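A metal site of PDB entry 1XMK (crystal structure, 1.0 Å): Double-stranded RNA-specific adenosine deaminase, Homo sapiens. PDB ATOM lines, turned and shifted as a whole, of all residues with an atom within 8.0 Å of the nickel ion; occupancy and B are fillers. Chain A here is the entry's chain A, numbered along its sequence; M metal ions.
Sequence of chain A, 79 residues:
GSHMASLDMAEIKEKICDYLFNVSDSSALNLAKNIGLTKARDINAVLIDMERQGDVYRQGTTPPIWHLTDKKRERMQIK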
ATOM      1  N   GLY A   1     -17.407 -22.750 -16.373  1.00  0.00           N
ATOM      2  CA  GLY A   1     -16.097 -23.201 -16.898  1.00  0.00           C
ATOM      3  C   GLY A   1     -15.165 -21.986 -16.876  1.00  0.00           C
ATOM      4  O   GLY A   1     -13.957 -21.999 -17.054  1.00  0.00           O
ATOM      5  N   SER A   2     -15.847 -20.894 -16.585  1.00  0.00           N
ATOM      6  CA  SER A   2     -15.289 -19.566 -16.635  1.00  0.00           C
ATOM      7  C   SER A   2     -16.152 -18.620 -15.808  1.00  0.00           C
ATOM      8  O   SER A   2     -15.730 -17.466 -15.556  1.00  0.00           O
ATOM      9  CB  SER A   2     -15.223 -19.023 -18.083  1.00  0.00           C
ATOM     10  OG  SER A   2     -16.526 -19.135 -18.681  1.00  0.00           O
ATOM     11  N   HIS A   3     -17.340 -19.146 -15.429  1.00  0.00           N
ATOM     12  CA  HIS A   3     -18.323 -18.190 -14.905  1.00  0.00           C
ATOM     13  C   HIS A   3     -18.155 -18.114 -13.383  1.00  0.00           C
ATOM     14  O   HIS A   3     -19.196 -18.331 -12.739  1.00  0.00           O
ATOM     15  CB  HIS A   3     -19.757 -18.544 -15.303  1.00  0.00           C
ATOM     16  CG  HIS A   3     -20.154 -19.984 -15.022  1.00  0.00           C
ATOM     17  ND1 HIS A   3     -19.326 -21.029 -15.245  1.00  0.00           N
ATOM     18  CD2 HIS A   3     -21.381 -20.455 -14.559  1.00  0.00           C
ATOM     19  CE1 HIS A   3     -19.978 -22.165 -14.923  1.00  0.00           C
ATOM     20  NE2 HIS A   3     -21.209 -21.841 -14.504  1.00  0.00           N
ATOM     21  N   MET A   4     -16.925 -17.812 -12.958  1.00  0.00           N
ATOM     22  CA  MET A   4     -16.555 -17.670 -11.563  1.00  0.00           C
ATOM     23  C   MET A   4     -17.440 -16.708 -10.787  1.00  0.00           C
ATOM     24  O   MET A   4     -17.502 -16.855  -9.562  1.00  0.00           O
ATOM     25  CB  MET A   4     -15.109 -17.228 -11.353  1.00  0.00           C
ATOM     26  CG  MET A   4     -14.027 -18.088 -11.966  1.00  0.00           C
ATOM     27  SD  MET A   4     -14.199 -19.733 -11.253  1.00  0.00           S
ATOM     28  CE  MET A   4     -14.433 -19.425  -9.506  1.00  0.00           C
ATOM     29  N   ALA A   5     -18.124 -15.729 -11.427  1.00  0.00           N
ATOM     30  CA  ALA A   5     -18.973 -14.809 -10.700  1.00  0.00           C
ATOM     31  C   ALA A   5     -20.407 -15.321 -10.457  1.00  0.00           C
ATOM     32  O   ALA A   5     -21.166 -14.623  -9.785  1.00  0.00           O
ATOM     33  CB  ALA A   5     -19.016 -13.503 -11.515  1.00  0.00           C
ATOM     34  N   SER A   6     -20.785 -16.474 -11.016  1.00  0.00           N
ATOM     35  CA  SER A   6     -22.157 -16.987 -10.846  1.00  0.00           C
ATOM     36  C   SER A   6     -22.416 -17.586  -9.491  1.00  0.00           C
ATOM     37  O   SER A   6     -21.540 -18.049  -8.788  1.00  0.00           O
ATOM     38  CB  SER A   6     -22.405 -18.031 -11.973  1.00  0.00           C
ATOM     39  OG  SER A   6     -21.720 -19.246 -11.648  1.00  0.00           O
ATOM     40  N   MET A   9     -21.136 -21.154  -9.428  1.00  0.00           N
ATOM     41  CA  MET A   9     -19.706 -21.361  -9.138  1.00  0.00           C
ATOM     42  C   MET A   9     -19.383 -21.017  -7.708  1.00  0.00           C
ATOM     43  O   MET A   9     -18.488 -21.637  -7.134  1.00  0.00           O
ATOM     44  CB  MET A   9     -18.864 -20.585 -10.142  1.00  0.00           C
ATOM     45  CG  MET A   9     -18.937 -21.158 -11.564  1.00  0.00           C
ATOM     46  SD  MET A   9     -18.249 -22.806 -11.721  1.00  0.00           S
ATOM     47  CE  MET A   9     -16.660 -22.412 -12.415  1.00  0.00           C
ATOM     48  N   ARG A  41     -15.962 -30.420 -14.536  1.00  0.00           N
ATOM     49  CA  ARG A  41     -15.229 -29.336 -15.227  1.00  0.00           C
ATOM     50  C   ARG A  41     -15.277 -28.052 -14.422  1.00  0.00           C
ATOM     51  O   ARG A  41     -14.291 -27.308 -14.371  1.00  0.00           O
ATOM     52  CB  ARG A  41     -15.803 -29.231 -16.638  1.00  0.00           C
ATOM     53  CG  ARG A  41     -14.952 -28.367 -17.562  1.00  0.00           C
ATOM     54  CD  ARG A  41     -15.497 -28.365 -18.984  1.00  0.00           C
ATOM     55  NE  ARG A  41     -14.877 -27.267 -19.736  1.00  0.00           N
ATOM     56  CZ  ARG A  41     -13.620 -27.312 -20.214  1.00  0.00           C
ATOM     57  NH1 ARG A  41     -12.871 -28.411 -20.034  1.00  0.00           N
ATOM     58  NH2 ARG A  41     -13.121 -26.300 -20.874  1.00  0.00           N
ATOM     59  N   ASP A  42     -16.411 -27.758 -13.748  1.00  0.00           N
ATOM     60  CA  ASP A  42     -16.453 -26.529 -12.930  1.00  0.00           C
ATOM     61  C   ASP A  42     -15.579 -26.663 -11.689  1.00  0.00           C
ATOM     62  O   ASP A  42     -14.952 -25.693 -11.258  1.00  0.00           O
ATOM     63  CB  ASP A  42     -17.887 -26.216 -12.576  1.00  0.00           C
ATOM     64  CG  ASP A  42     -18.585 -25.618 -13.797  1.00  0.00           C
ATOM     65  OD1 ASP A  42     -17.967 -24.986 -14.703  1.00  0.00           O
ATOM     66  OD2 ASP A  42     -19.791 -25.774 -13.884  1.00  0.00           O
ATOM     67  N   ALA A  45     -12.142 -25.929 -12.831  1.00  0.00           N
ATOM     68  CA  ALA A  45     -11.967 -24.496 -13.106  1.00  0.00           C
ATOM     69  C   ALA A  45     -11.844 -23.693 -11.811  1.00  0.00           C
ATOM     70  O   ALA A  45     -10.998 -22.763 -11.738  1.00  0.00           O
ATOM     71  CB  ALA A  45     -13.170 -24.037 -13.931  1.00  0.00           C
ATOM     72  N   VAL A  46     -12.619 -24.008 -10.793  1.00  0.00           N
ATOM     73  CA  VAL A  46     -12.516 -23.317  -9.511  1.00  0.00           C
ATOM     74  C   VAL A  46     -11.152 -23.620  -8.856  1.00  0.00           C
ATOM     75  O   VAL A  46     -10.519 -22.700  -8.355  1.00  0.00           O
ATOM     76  CB  VAL A  46     -13.666 -23.701  -8.550  1.00  0.00           C
ATOM     77  CG1 VAL A  46     -13.436 -23.166  -7.131  1.00  0.00           C
ATOM     78  CG2 VAL A  46     -15.017 -23.183  -9.081  1.00  0.00           C
HETATM   79 NI    NI M   1     -17.504 -20.920 -15.883  1.00  0.00          NI
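Met 9 touches the nickel ion (CE to NI, 3.9 Å).
Four residues have an atom within 4 Å of the nickel ion: Gly 1, Ser 2, His 3 and Met 9.
The nickel ion is bound by the backbone nitrogen of Ser 2 (1.8 Å), the backbone nitrogen of His 3 (1.8 Å), the backbone nitrogen of Gly 1 (1.9 Å) and a ring nitrogen (ND1) of His 3 (1.9 Å).
The nickel ion has four donor atoms within binding distance.
The backbone carbonyl oxygen (O) of His 3 sits at hydrogen-bond distance from the side-chain hydroxyl (OG) of Ser 6 (2.9 Å).
The side-chain carboxylate (OD1) of Asp 42 sits close to the backbone NH (N) of Gly 1 (2.8 Å).
The side-chain hydroxyl (OG) of Ser 6 lies within hydrogen-bond range of the backbone NH (N) of Met 9 (3.0 Å).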
